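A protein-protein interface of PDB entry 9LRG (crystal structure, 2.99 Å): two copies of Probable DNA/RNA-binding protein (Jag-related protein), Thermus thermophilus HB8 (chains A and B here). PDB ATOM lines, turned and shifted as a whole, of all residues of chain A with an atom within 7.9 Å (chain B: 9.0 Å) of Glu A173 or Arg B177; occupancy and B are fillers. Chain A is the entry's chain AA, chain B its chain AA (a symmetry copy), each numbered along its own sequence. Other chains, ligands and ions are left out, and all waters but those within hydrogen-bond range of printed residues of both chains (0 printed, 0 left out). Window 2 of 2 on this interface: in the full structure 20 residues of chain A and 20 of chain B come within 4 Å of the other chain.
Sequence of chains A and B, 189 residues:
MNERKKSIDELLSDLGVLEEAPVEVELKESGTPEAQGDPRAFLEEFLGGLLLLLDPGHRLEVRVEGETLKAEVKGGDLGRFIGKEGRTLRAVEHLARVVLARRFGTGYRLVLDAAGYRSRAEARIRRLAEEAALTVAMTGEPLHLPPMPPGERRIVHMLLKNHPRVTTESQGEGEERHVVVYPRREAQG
The guanidinium group (NH2) of Arg A177 is in salt-bridge range of the side-chain carboxylate (OE2) of Glu B173 (2.5 Å). The side-chain carboxylate (OE2) of Glu A173 is in salt-bridge range of the guanidinium group (NH2) of Arg B177 (2.5 Å). OE1 of Glu B173 lies within salt-bridge range of NH2 of Arg A153 (2.5 Å). NH2 of Arg A154 is in salt-bridge range of OE2 of Glu B173. The guanidinium group of Arg A177 lies close to the guanidinium group of Arg B177 (3.3 Å). NH2 of Arg B153 lies within salt-bridge range of OE1 of Glu A173 (2.5 Å). The guanidinium group (NH2) of Arg B154 lies within salt-bridge range of the side-chain carboxylate (OE2) of Glu A173 (3.5 Å).
The side-chain hydroxyl (OG) of Ser A170 sits at hydrogen-bond distance from the guanidinium group (NH2) of Arg A154, 2.8 Å away. The guanidinium group (NH1) of Arg A177 is in hydrogen-bond range of the backbone carbonyl oxygen (O) of Gly A172, 2.6 Å away. NH1 of Arg B153 sits at hydrogen-bond distance from O of Met B148, at 2.9 Å. OG of Ser B170 is in hydrogen-bond range of NH2 of Arg B154 (2.8 Å). The guanidinium group of Arg B177 lies within hydrogen-bond range of the backbone carbonyl oxygen of Gly B172 (2.6 Å). The side-chain carboxylate (OE2) of Glu A173 lies within salt-bridge range of the guanidinium group (NH1) of Arg A177.
Among the printed residues, pairs that only touch across the chains: Gly A174 with Pro B150 (3.6 Å).
Of the printed residues of chain B, Glu A173 touches Arg B153 (2.5 Å), Arg B154 (3.3 Å) and Arg B177 (2.5 Å). No residue of chain B comes within 4 Å of Gly A172. Printed residues of chain A within 4 Å of Arg B153: Glu A173 (2.5 Å). Of the printed residues of chain A, Arg B154 touches Glu A173. Of the printed residues of chain A, Glu B173 touches Arg A153 (2.5 Å), Arg A154 (3.3 Å) and Arg A177 (2.5 Å). Glu A175 touches none of the printed residues of chain B. The nearest printed residue of chain A that does not touch Arg B154 is Gly A172 (6.6 Å).
Printed residues of chain A that touch a printed residue of chain B: Arg A153, Arg A154, Glu A173, Gly A174 and Arg A177. Hydrophobic or aromatic side chains of chain B that line the printed part of chain A: Pro B150. Along chain B the printed residues that touch a printed residue of chain A span positions 150 to 177. Among the printed residues, 8 pairs touch across the chains. Among the printed residues, Asp or Glu carboxylates within 4 Å of a Lys or Arg side-chain nitrogen of the other chain: Arg A153 with Glu B173, Arg A154 with Glu B173, Glu A173 with Arg B153, Glu A173 with Arg B154, Glu A173 with Arg B177 and Arg A177 with Glu B173.
Arg A153 touches Glu B173, and with the chains exchanged Glu A173 touches Arg B153. Arg A154 touches Glu B173, and with the chains exchanged Glu A173 touches Arg B154. Glu A173 touches Arg B177, and with the chains exchanged Arg A177 touches Glu B173. Arg B177 touches its own counterpart, Arg A177. Positions printed for both chains: 147, 153, 154, 170, 171, 172, 173, 174, 175, 176, 177 and 178.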
ATOM      1  N   PRO A 147      18.512 -20.190  14.303  1.00  0.00           N
ATOM      2  CA  PRO A 147      18.013 -18.866  14.688  1.00  0.00           C
ATOM      3  C   PRO A 147      18.895 -17.762  14.132  1.00  0.00           C
ATOM      4  O   PRO A 147      20.126 -17.838  14.174  1.00  0.00           O
ATOM      5  CB  PRO A 147      18.056 -18.902  16.220  1.00  0.00           C
ATOM      6  CG  PRO A 147      18.034 -20.347  16.570  1.00  0.00           C
ATOM      7  CD  PRO A 147      18.782 -21.043  15.473  1.00  0.00           C
ATOM      8  N   ARG A 153      16.322 -13.008   8.554  1.00  0.00           N
ATOM      9  CA  ARG A 153      15.140 -13.816   8.280  1.00  0.00           C
ATOM     10  C   ARG A 153      14.372 -13.280   7.078  1.00  0.00           C
ATOM     11  O   ARG A 153      13.889 -14.058   6.247  1.00  0.00           O
ATOM     12  CB  ARG A 153      14.235 -13.873   9.511  1.00  0.00           C
ATOM     13  CG  ARG A 153      14.857 -14.563  10.712  1.00  0.00           C
ATOM     14  CD  ARG A 153      13.797 -15.003  11.712  1.00  0.00           C
ATOM     15  NE  ARG A 153      12.979 -13.893  12.186  1.00  0.00           N
ATOM     16  CZ  ARG A 153      13.241 -13.177  13.271  1.00  0.00           C
ATOM     17  NH1 ARG A 153      14.306 -13.418  14.018  1.00  0.00           N
ATOM     18  NH2 ARG A 153      12.412 -12.197  13.618  1.00  0.00           N
ATOM     19  N   ARG A 154      14.251 -11.955   6.967  1.00  0.00           N
ATOM     20  CA  ARG A 154      13.541 -11.375   5.832  1.00  0.00           C
ATOM     21  C   ARG A 154      14.257 -11.662   4.520  1.00  0.00           C
ATOM     22  O   ARG A 154      13.609 -11.780   3.473  1.00  0.00           O
ATOM     23  CB  ARG A 154      13.370  -9.867   6.026  1.00  0.00           C
ATOM     24  CG  ARG A 154      12.625  -9.471   7.292  1.00  0.00           C
ATOM     25  CD  ARG A 154      11.291 -10.197   7.419  1.00  0.00           C
ATOM     26  NE  ARG A 154      11.310 -11.185   8.492  1.00  0.00           N
ATOM     27  CZ  ARG A 154      10.269 -11.924   8.853  1.00  0.00           C
ATOM     28  NH1 ARG A 154       9.100 -11.817   8.243  1.00  0.00           N
ATOM     29  NH2 ARG A 154      10.404 -12.789   9.855  1.00  0.00           N
ATOM     30  N   SER A 170       8.113 -17.886   9.682  1.00  0.00           N
ATOM     31  CA  SER A 170       8.889 -17.607  10.882  1.00  0.00           C
ATOM     32  C   SER A 170       8.211 -18.234  12.093  1.00  0.00           C
ATOM     33  O   SER A 170       7.013 -18.032  12.318  1.00  0.00           O
ATOM     34  CB  SER A 170       9.048 -16.099  11.084  1.00  0.00           C
ATOM     35  OG  SER A 170       9.883 -15.538  10.087  1.00  0.00           O
ATOM     36  N   GLN A 171       8.980 -19.000  12.865  1.00  0.00           N
ATOM     37  CA  GLN A 171       8.489 -19.641  14.075  1.00  0.00           C
ATOM     38  C   GLN A 171       9.487 -19.425  15.203  1.00  0.00           C
ATOM     39  O   GLN A 171      10.678 -19.201  14.973  1.00  0.00           O
ATOM     40  CB  GLN A 171       8.248 -21.142  13.866  1.00  0.00           C
ATOM     41  CG  GLN A 171       7.207 -21.460  12.810  1.00  0.00           C
ATOM     42  CD  GLN A 171       7.119 -22.942  12.505  1.00  0.00           C
ATOM     43  OE1 GLN A 171       7.464 -23.782  13.335  1.00  0.00           O
ATOM     44  NE2 GLN A 171       6.661 -23.269  11.302  1.00  0.00           N
ATOM     45  N   GLY A 172       8.987 -19.503  16.432  1.00  0.00           N
ATOM     46  CA  GLY A 172       9.793 -19.248  17.606  1.00  0.00           C
ATOM     47  C   GLY A 172       9.667 -17.815  18.093  1.00  0.00           C
ATOM     48  O   GLY A 172       9.071 -16.948  17.452  1.00  0.00           O
ATOM     49  N   GLU A 173      10.252 -17.568  19.262  1.00  0.00           N
ATOM     50  CA  GLU A 173      10.189 -16.258  19.894  1.00  0.00           C
ATOM     51  C   GLU A 173      11.561 -15.863  20.415  1.00  0.00           C
ATOM     52  O   GLU A 173      12.314 -16.706  20.912  1.00  0.00           O
ATOM     53  CB  GLU A 173       9.171 -16.240  21.043  1.00  0.00           C
ATOM     54  CG  GLU A 173       7.724 -16.398  20.596  1.00  0.00           C
ATOM     55  CD  GLU A 173       7.247 -15.237  19.743  1.00  0.00           C
ATOM     56  OE1 GLU A 173       7.817 -14.131  19.861  1.00  0.00           O
ATOM     57  OE2 GLU A 173       6.303 -15.434  18.950  1.00  0.00           O
ATOM     58  N   GLY A 174      11.880 -14.577  20.296  1.00  0.00           N
ATOM     59  CA  GLY A 174      13.132 -14.074  20.840  1.00  0.00           C
ATOM     60  C   GLY A 174      14.328 -14.650  20.112  1.00  0.00           C
ATOM     61  O   GLY A 174      14.376 -14.689  18.877  1.00  0.00           O
ATOM     62  N   GLU A 175      15.312 -15.109  20.886  1.00  0.00           N
ATOM     63  CA  GLU A 175      16.517 -15.698  20.317  1.00  0.00           C
ATOM     64  C   GLU A 175      16.264 -17.047  19.660  1.00  0.00           C
ATOM     65  O   GLU A 175      17.169 -17.572  19.002  1.00  0.00           O
ATOM     66  CB  GLU A 175      17.587 -15.838  21.400  1.00  0.00           C
ATOM     67  CG  GLU A 175      18.268 -14.529  21.760  1.00  0.00           C
ATOM     68  CD  GLU A 175      18.882 -14.554  23.145  1.00  0.00           C
ATOM     69  OE1 GLU A 175      18.125 -14.445  24.133  1.00  0.00           O
ATOM     70  OE2 GLU A 175      20.120 -14.690  23.246  1.00  0.00           O
ATOM     71  N   GLU A 176      15.072 -17.620  19.818  1.00  0.00           N
ATOM     72  CA  GLU A 176      14.728 -18.874  19.165  1.00  0.00           C
ATOM     73  C   GLU A 176      13.950 -18.682  17.871  1.00  0.00           C
ATOM     74  O   GLU A 176      13.673 -19.670  17.183  1.00  0.00           O
ATOM     75  CB  GLU A 176      13.918 -19.765  20.115  1.00  0.00           C
ATOM     76  CG  GLU A 176      14.661 -20.154  21.379  1.00  0.00           C
ATOM     77  CD  GLU A 176      14.327 -21.561  21.839  1.00  0.00           C
ATOM     78  OE1 GLU A 176      13.420 -22.183  21.246  1.00  0.00           O
ATOM     79  OE2 GLU A 176      14.979 -22.048  22.787  1.00  0.00           O
ATOM     80  N   ARG A 177      13.597 -17.447  17.522  1.00  0.00           N
ATOM     81  CA  ARG A 177      12.826 -17.206  16.309  1.00  0.00           C
ATOM     82  C   ARG A 177      13.681 -17.494  15.081  1.00  0.00           C
ATOM     83  O   ARG A 177      14.819 -17.026  14.977  1.00  0.00           O
ATOM     84  CB  ARG A 177      12.311 -15.769  16.282  1.00  0.00           C
ATOM     85  CG  ARG A 177      11.280 -15.505  15.195  1.00  0.00           C
ATOM     86  CD  ARG A 177      10.352 -14.364  15.579  1.00  0.00           C
ATOM     87  NE  ARG A 177       9.296 -14.159  14.594  1.00  0.00           N
ATOM     88  CZ  ARG A 177       8.166 -14.850  14.549  1.00  0.00           C
ATOM     89  NH1 ARG A 177       7.912 -15.818  15.414  1.00  0.00           N
ATOM     90  NH2 ARG A 177       7.268 -14.567  13.609  1.00  0.00           N
ATOM     91  N   HIS A 178      13.130 -18.271  14.153  1.00  0.00           N
ATOM     92  CA  HIS A 178      13.877 -18.731  12.994  1.00  0.00           C
ATOM     93  C   HIS A 178      12.914 -18.943  11.835  1.00  0.00           C
ATOM     94  O   HIS A 178      11.693 -18.858  11.989  1.00  0.00           O
ATOM     95  CB  HIS A 178      14.638 -20.022  13.306  1.00  0.00           C
ATOM     96  CG  HIS A 178      13.749 -21.161  13.694  1.00  0.00           C
ATOM     97  ND1 HIS A 178      13.207 -21.287  14.955  1.00  0.00           N
ATOM     98  CD2 HIS A 178      13.297 -22.221  12.983  1.00  0.00           C
ATOM     99  CE1 HIS A 178      12.464 -22.379  15.005  1.00  0.00           C
ATOM    100  NE2 HIS A 178      12.502 -22.963  13.821  1.00  0.00           N
ATOM    101  N   HIS B 144      -3.691  -3.451  19.426  1.00  0.00           N
ATOM    102  CA  HIS B 144      -2.280  -3.812  19.345  1.00  0.00           C
ATOM    103  C   HIS B 144      -1.559  -3.238  20.559  1.00  0.00           C
ATOM    104  O   HIS B 144      -1.398  -2.019  20.676  1.00  0.00           O
ATOM    105  CB  HIS B 144      -1.668  -3.301  18.043  1.00  0.00           C
ATOM    106  CG  HIS B 144      -2.267  -3.912  16.815  1.00  0.00           C
ATOM    107  ND1 HIS B 144      -1.601  -4.841  16.044  1.00  0.00           N
ATOM    108  CD2 HIS B 144      -3.472  -3.730  16.225  1.00  0.00           C
ATOM    109  CE1 HIS B 144      -2.369  -5.203  15.033  1.00  0.00           C
ATOM    110  NE2 HIS B 144      -3.510  -4.545  15.119  1.00  0.00           N
ATOM    111  N   LEU B 145      -1.132  -4.115  21.466  1.00  0.00           N
ATOM    112  CA  LEU B 145      -0.380  -3.686  22.631  1.00  0.00           C
ATOM    113  C   LEU B 145       0.972  -3.116  22.208  1.00  0.00           C
ATOM    114  O   LEU B 145       1.455  -3.394  21.106  1.00  0.00           O
ATOM    115  CB  LEU B 145      -0.184  -4.854  23.594  1.00  0.00           C
ATOM    116  CG  LEU B 145      -1.431  -5.347  24.327  1.00  0.00           C
ATOM    117  CD1 LEU B 145      -1.098  -6.543  25.206  1.00  0.00           C
ATOM    118  CD2 LEU B 145      -2.038  -4.225  25.152  1.00  0.00           C
ATOM    119  N   PRO B 146       1.594  -2.304  23.059  1.00  0.00           N
ATOM    120  CA  PRO B 146       2.910  -1.773  22.722  1.00  0.00           C
ATOM    121  C   PRO B 146       3.924  -2.891  22.606  1.00  0.00           C
ATOM    122  O   PRO B 146       3.750  -3.978  23.191  1.00  0.00           O
ATOM    123  CB  PRO B 146       3.229  -0.842  23.900  1.00  0.00           C
ATOM    124  CG  PRO B 146       1.906  -0.479  24.465  1.00  0.00           C
ATOM    125  CD  PRO B 146       1.056  -1.700  24.291  1.00  0.00           C
ATOM    126  N   PRO B 147       4.997  -2.679  21.847  1.00  0.00           N
ATOM    127  CA  PRO B 147       6.041  -3.703  21.743  1.00  0.00           C
ATOM    128  C   PRO B 147       6.691  -3.966  23.090  1.00  0.00           C
ATOM    129  O   PRO B 147       7.004  -3.042  23.845  1.00  0.00           O
ATOM    130  CB  PRO B 147       7.036  -3.097  20.747  1.00  0.00           C
ATOM    131  CG  PRO B 147       6.248  -2.097  19.979  1.00  0.00           C
ATOM    132  CD  PRO B 147       5.245  -1.542  20.944  1.00  0.00           C
ATOM    133  N   MET B 148       6.889  -5.243  23.386  1.00  0.00           N
ATOM    134  CA  MET B 148       7.479  -5.662  24.644  1.00  0.00           C
ATOM    135  C   MET B 148       8.322  -6.901  24.390  1.00  0.00           C
ATOM    136  O   MET B 148       8.104  -7.614  23.403  1.00  0.00           O
ATOM    137  CB  MET B 148       6.400  -5.931  25.703  1.00  0.00           C
ATOM    138  CG  MET B 148       5.150  -6.621  25.193  1.00  0.00           C
ATOM    139  SD  MET B 148       3.783  -6.504  26.368  1.00  0.00           S
ATOM    140  CE  MET B 148       3.492  -4.737  26.380  1.00  0.00           C
ATOM    141  N   PRO B 149       9.306  -7.169  25.241  1.00  0.00           N
ATOM    142  CA  PRO B 149      10.195  -8.317  25.031  1.00  0.00           C
ATOM    143  C   PRO B 149       9.437  -9.629  25.132  1.00  0.00           C
ATOM    144  O   PRO B 149       8.297  -9.660  25.621  1.00  0.00           O
ATOM    145  CB  PRO B 149      11.224  -8.174  26.166  1.00  0.00           C
ATOM    146  CG  PRO B 149      10.550  -7.313  27.189  1.00  0.00           C
ATOM    147  CD  PRO B 149       9.714  -6.363  26.402  1.00  0.00           C
ATOM    148  N   PRO B 150      10.035 -10.737  24.679  1.00  0.00           N
ATOM    149  CA  PRO B 150       9.316 -12.023  24.714  1.00  0.00           C
ATOM    150  C   PRO B 150       8.872 -12.445  26.104  1.00  0.00           C
ATOM    151  O   PRO B 150       7.816 -13.076  26.240  1.00  0.00           O
ATOM    152  CB  PRO B 150      10.337 -13.008  24.127  1.00  0.00           C
ATOM    153  CG  PRO B 150      11.232 -12.166  23.289  1.00  0.00           C
ATOM    154  CD  PRO B 150      11.337 -10.852  23.999  1.00  0.00           C
ATOM    155  N   GLY B 151       9.647 -12.121  27.141  1.00  0.00           N
ATOM    156  CA  GLY B 151       9.255 -12.502  28.487  1.00  0.00           C
ATOM    157  C   GLY B 151       7.950 -11.861  28.921  1.00  0.00           C
ATOM    158  O   GLY B 151       7.114 -12.505  29.560  1.00  0.00           O
ATOM    159  N   GLU B 152       7.756 -10.587  28.578  1.00  0.00           N
ATOM    160  CA  GLU B 152       6.521  -9.902  28.936  1.00  0.00           C
ATOM    161  C   GLU B 152       5.359 -10.305  28.037  1.00  0.00           C
ATOM    162  O   GLU B 152       4.202 -10.249  28.469  1.00  0.00           O
ATOM    163  CB  GLU B 152       6.723  -8.386  28.885  1.00  0.00           C
ATOM    164  CG  GLU B 152       7.700  -7.857  29.922  1.00  0.00           C
ATOM    165  CD  GLU B 152       7.853  -6.350  29.866  1.00  0.00           C
ATOM    166  OE1 GLU B 152       7.393  -5.739  28.878  1.00  0.00           O
ATOM    167  OE2 GLU B 152       8.429  -5.776  30.813  1.00  0.00           O
ATOM    168  N   ARG B 153       5.639 -10.710  26.796  1.00  0.00           N
ATOM    169  CA  ARG B 153       4.567 -11.141  25.907  1.00  0.00           C
ATOM    170  C   ARG B 153       3.940 -12.443  26.388  1.00  0.00           C
ATOM    171  O   ARG B 153       2.715 -12.604  26.337  1.00  0.00           O
ATOM    172  CB  ARG B 153       5.089 -11.294  24.478  1.00  0.00           C
ATOM    173  CG  ARG B 153       5.568 -10.000  23.845  1.00  0.00           C
ATOM    174  CD  ARG B 153       5.626 -10.109  22.327  1.00  0.00           C
ATOM    175  NE  ARG B 153       6.492 -11.194  21.878  1.00  0.00           N
ATOM    176  CZ  ARG B 153       7.779 -11.058  21.593  1.00  0.00           C
ATOM    177  NH1 ARG B 153       8.396  -9.894  21.715  1.00  0.00           N
ATOM    178  NH2 ARG B 153       8.466 -12.117  21.173  1.00  0.00           N
ATOM    179  N   ARG B 154       4.762 -13.383  26.861  1.00  0.00           N
ATOM    180  CA  ARG B 154       4.226 -14.649  27.352  1.00  0.00           C
ATOM    181  C   ARG B 154       3.358 -14.445  28.585  1.00  0.00           C
ATOM    182  O   ARG B 154       2.407 -15.204  28.806  1.00  0.00           O
ATOM    183  CB  ARG B 154       5.362 -15.626  27.656  1.00  0.00           C
ATOM    184  CG  ARG B 154       6.269 -15.933  26.474  1.00  0.00           C
ATOM    185  CD  ARG B 154       5.477 -16.375  25.249  1.00  0.00           C
ATOM    186  NE  ARG B 154       5.496 -15.365  24.196  1.00  0.00           N
ATOM    187  CZ  ARG B 154       4.931 -15.510  23.005  1.00  0.00           C
ATOM    188  NH1 ARG B 154       4.282 -16.614  22.677  1.00  0.00           N
ATOM    189  NH2 ARG B 154       5.021 -14.521  22.120  1.00  0.00           N
ATOM    190  N   HIS B 157       0.028 -13.455  27.274  1.00  0.00           N
ATOM    191  CA  HIS B 157      -0.637 -14.655  26.775  1.00  0.00           C
ATOM    192  C   HIS B 157      -1.102 -15.544  27.921  1.00  0.00           C
ATOM    193  O   HIS B 157      -2.201 -16.110  27.868  1.00  0.00           O
ATOM    194  CB  HIS B 157       0.299 -15.430  25.846  1.00  0.00           C
ATOM    195  CG  HIS B 157       0.544 -14.756  24.532  1.00  0.00           C
ATOM    196  ND1 HIS B 157      -0.438 -14.610  23.577  1.00  0.00           N
ATOM    197  CD2 HIS B 157       1.663 -14.204  24.007  1.00  0.00           C
ATOM    198  CE1 HIS B 157       0.063 -13.988  22.524  1.00  0.00           C
ATOM    199  NE2 HIS B 157       1.336 -13.730  22.760  1.00  0.00           N
ATOM    200  N   GLU B 169      -2.496 -13.011  20.298  1.00  0.00           N
ATOM    201  CA  GLU B 169      -1.661 -13.471  19.196  1.00  0.00           C
ATOM    202  C   GLU B 169      -0.497 -12.507  19.037  1.00  0.00           C
ATOM    203  O   GLU B 169      -0.693 -11.288  19.063  1.00  0.00           O
ATOM    204  CB  GLU B 169      -2.470 -13.564  17.897  1.00  0.00           C
ATOM    205  CG  GLU B 169      -1.722 -14.191  16.733  1.00  0.00           C
ATOM    206  CD  GLU B 169      -2.617 -14.432  15.531  1.00  0.00           C
ATOM    207  OE1 GLU B 169      -3.763 -13.937  15.535  1.00  0.00           O
ATOM    208  OE2 GLU B 169      -2.176 -15.124  14.588  1.00  0.00           O
ATOM    209  N   SER B 170       0.706 -13.052  18.881  1.00  0.00           N
ATOM    210  CA  SER B 170       1.905 -12.247  18.702  1.00  0.00           C
ATOM    211  C   SER B 170       2.077 -11.897  17.229  1.00  0.00           C
ATOM    212  O   SER B 170       2.038 -12.779  16.364  1.00  0.00           O
ATOM    213  CB  SER B 170       3.138 -12.990  19.219  1.00  0.00           C
ATOM    214  OG  SER B 170       3.105 -13.110  20.629  1.00  0.00           O
ATOM    215  N   GLN B 171       2.261 -10.607  16.949  1.00  0.00           N
ATOM    216  CA  GLN B 171       2.473 -10.120  15.595  1.00  0.00           C
ATOM    217  C   GLN B 171       3.642  -9.145  15.586  1.00  0.00           C
ATOM    218  O   GLN B 171       3.975  -8.532  16.603  1.00  0.00           O
ATOM    219  CB  GLN B 171       1.218  -9.440  15.031  1.00  0.00           C
ATOM    220  CG  GLN B 171       0.013 -10.356  14.928  1.00  0.00           C
ATOM    221  CD  GLN B 171      -1.250  -9.617  14.535  1.00  0.00           C
ATOM    222  OE1 GLN B 171      -1.196  -8.557  13.911  1.00  0.00           O
ATOM    223  NE2 GLN B 171      -2.396 -10.171  14.909  1.00  0.00           N
ATOM    224  N   GLY B 172       4.260  -9.003  14.418  1.00  0.00           N
ATOM    225  CA  GLY B 172       5.433  -8.171  14.266  1.00  0.00           C
ATOM    226  C   GLY B 172       6.722  -8.964  14.380  1.00  0.00           C
ATOM    227  O   GLY B 172       6.744 -10.147  14.724  1.00  0.00           O
ATOM    228  N   GLU B 173       7.827  -8.284  14.084  1.00  0.00           N
ATOM    229  CA  GLU B 173       9.143  -8.905  14.098  1.00  0.00           C
ATOM    230  C   GLU B 173      10.141  -7.998  14.801  1.00  0.00           C
ATOM    231  O   GLU B 173      10.084  -6.773  14.664  1.00  0.00           O
ATOM    232  CB  GLU B 173       9.632  -9.214  12.676  1.00  0.00           C
ATOM    233  CG  GLU B 173       8.830 -10.292  11.962  1.00  0.00           C
ATOM    234  CD  GLU B 173       8.950 -11.649  12.631  1.00  0.00           C
ATOM    235  OE1 GLU B 173       9.959 -11.887  13.327  1.00  0.00           O
ATOM    236  OE2 GLU B 173       8.030 -12.476  12.460  1.00  0.00           O
ATOM    237  N   GLY B 174      11.050  -8.610  15.554  1.00  0.00           N
ATOM    238  CA  GLY B 174      12.106  -7.845  16.202  1.00  0.00           C
ATOM    239  C   GLY B 174      11.551  -6.916  17.262  1.00  0.00           C
ATOM    240  O   GLY B 174      10.724  -7.305  18.094  1.00  0.00           O
ATOM    241  N   GLU B 175      12.011  -5.665  17.233  1.00  0.00           N
ATOM    242  CA  GLU B 175      11.556  -4.664  18.189  1.00  0.00           C
ATOM    243  C   GLU B 175      10.108  -4.249  17.969  1.00  0.00           C
ATOM    244  O   GLU B 175       9.556  -3.530  18.808  1.00  0.00           O
ATOM    245  CB  GLU B 175      12.464  -3.437  18.128  1.00  0.00           C
ATOM    246  CG  GLU B 175      13.805  -3.635  18.812  1.00  0.00           C
ATOM    247  CD  GLU B 175      14.870  -2.689  18.294  1.00  0.00           C
ATOM    248  OE1 GLU B 175      15.389  -2.928  17.183  1.00  0.00           O
ATOM    249  OE2 GLU B 175      15.182  -1.701  18.994  1.00  0.00           O
ATOM    250  N   GLU B 176       9.483  -4.674  16.871  1.00  0.00           N
ATOM    251  CA  GLU B 176       8.080  -4.380  16.622  1.00  0.00           C
ATOM    252  C   GLU B 176       7.148  -5.511  17.034  1.00  0.00           C
ATOM    253  O   GLU B 176       5.926  -5.346  16.946  1.00  0.00           O
ATOM    254  CB  GLU B 176       7.858  -4.056  15.140  1.00  0.00           C
ATOM    255  CG  GLU B 176       8.623  -2.839  14.654  1.00  0.00           C
ATOM    256  CD  GLU B 176       7.848  -2.041  13.622  1.00  0.00           C
ATOM    257  OE1 GLU B 176       6.772  -2.508  13.190  1.00  0.00           O
ATOM    258  OE2 GLU B 176       8.310  -0.941  13.249  1.00  0.00           O
ATOM    259  N   ARG B 177       7.686  -6.645  17.478  1.00  0.00           N
ATOM    260  CA  ARG B 177       6.844  -7.772  17.858  1.00  0.00           C
ATOM    261  C   ARG B 177       6.069  -7.440  19.127  1.00  0.00           C
ATOM    262  O   ARG B 177       6.641  -6.968  20.114  1.00  0.00           O
ATOM    263  CB  ARG B 177       7.691  -9.027  18.057  1.00  0.00           C
ATOM    264  CG  ARG B 177       6.876 -10.304  18.190  1.00  0.00           C
ATOM    265  CD  ARG B 177       7.673 -11.517  17.738  1.00  0.00           C
ATOM    266  NE  ARG B 177       6.878 -12.739  17.768  1.00  0.00           N
ATOM    267  CZ  ARG B 177       6.053 -13.123  16.803  1.00  0.00           C
ATOM    268  NH1 ARG B 177       5.875 -12.391  15.715  1.00  0.00           N
ATOM    269  NH2 ARG B 177       5.385 -14.265  16.935  1.00  0.00           N
ATOM    270  N   HIS B 178       4.762  -7.683  19.096  1.00  0.00           N
ATOM    271  CA  HIS B 178       3.881  -7.297  20.186  1.00  0.00           C
ATOM    272  C   HIS B 178       2.705  -8.260  20.240  1.00  0.00           C
ATOM    273  O   HIS B 178       2.530  -9.112  19.365  1.00  0.00           O
ATOM    274  CB  HIS B 178       3.393  -5.856  20.015  1.00  0.00           C
ATOM    275  CG  HIS B 178       2.604  -5.639  18.760  1.00  0.00           C
ATOM    276  ND1 HIS B 178       3.198  -5.484  17.526  1.00  0.00           N
ATOM    277  CD2 HIS B 178       1.270  -5.559  18.549  1.00  0.00           C
ATOM    278  CE1 HIS B 178       2.261  -5.314  16.609  1.00  0.00           C
ATOM    279  NE2 HIS B 178       1.084  -5.357  17.204  1.00  0.00           N
ATOM    280  N   VAL B 179       1.890  -8.108  21.281  1.00  0.00           N
ATOM    281  CA  VAL B 179       0.696  -8.922  21.485  1.00  0.00           C
ATOM    282  C   VAL B 179      -0.512  -8.156  20.967  1.00  0.00           C
ATOM    283  O   VAL B 179      -0.642  -6.948  21.197  1.00  0.00           O
ATOM    284  CB  VAL B 179       0.520  -9.291  22.970  1.00  0.00           C
ATOM    285  CG1 VAL B 179      -0.703 -10.175  23.158  1.00  0.00           C
ATOM    286  CG2 VAL B 179       1.768  -9.978  23.500  1.00  0.00           C
ATOM    287  N   VAL B 180      -1.397  -8.857  20.263  1.00  0.00           N
ATOM    288  CA  VAL B 180      -2.632  -8.284  19.741  1.00  0.00           C
ATOM    289  C   VAL B 180      -3.800  -8.993  20.408  1.00  0.00           C
ATOM    290  O   VAL B 180      -3.868 -10.228  20.406  1.00  0.00           O
ATOM    291  CB  VAL B 180      -2.715  -8.409  18.209  1.00  0.00           C
ATOM    292  CG1 VAL B 180      -3.955  -7.706  17.685  1.00  0.00           C
ATOM    293  CG2 VAL B 180      -1.457  -7.843  17.563  1.00  0.00           C
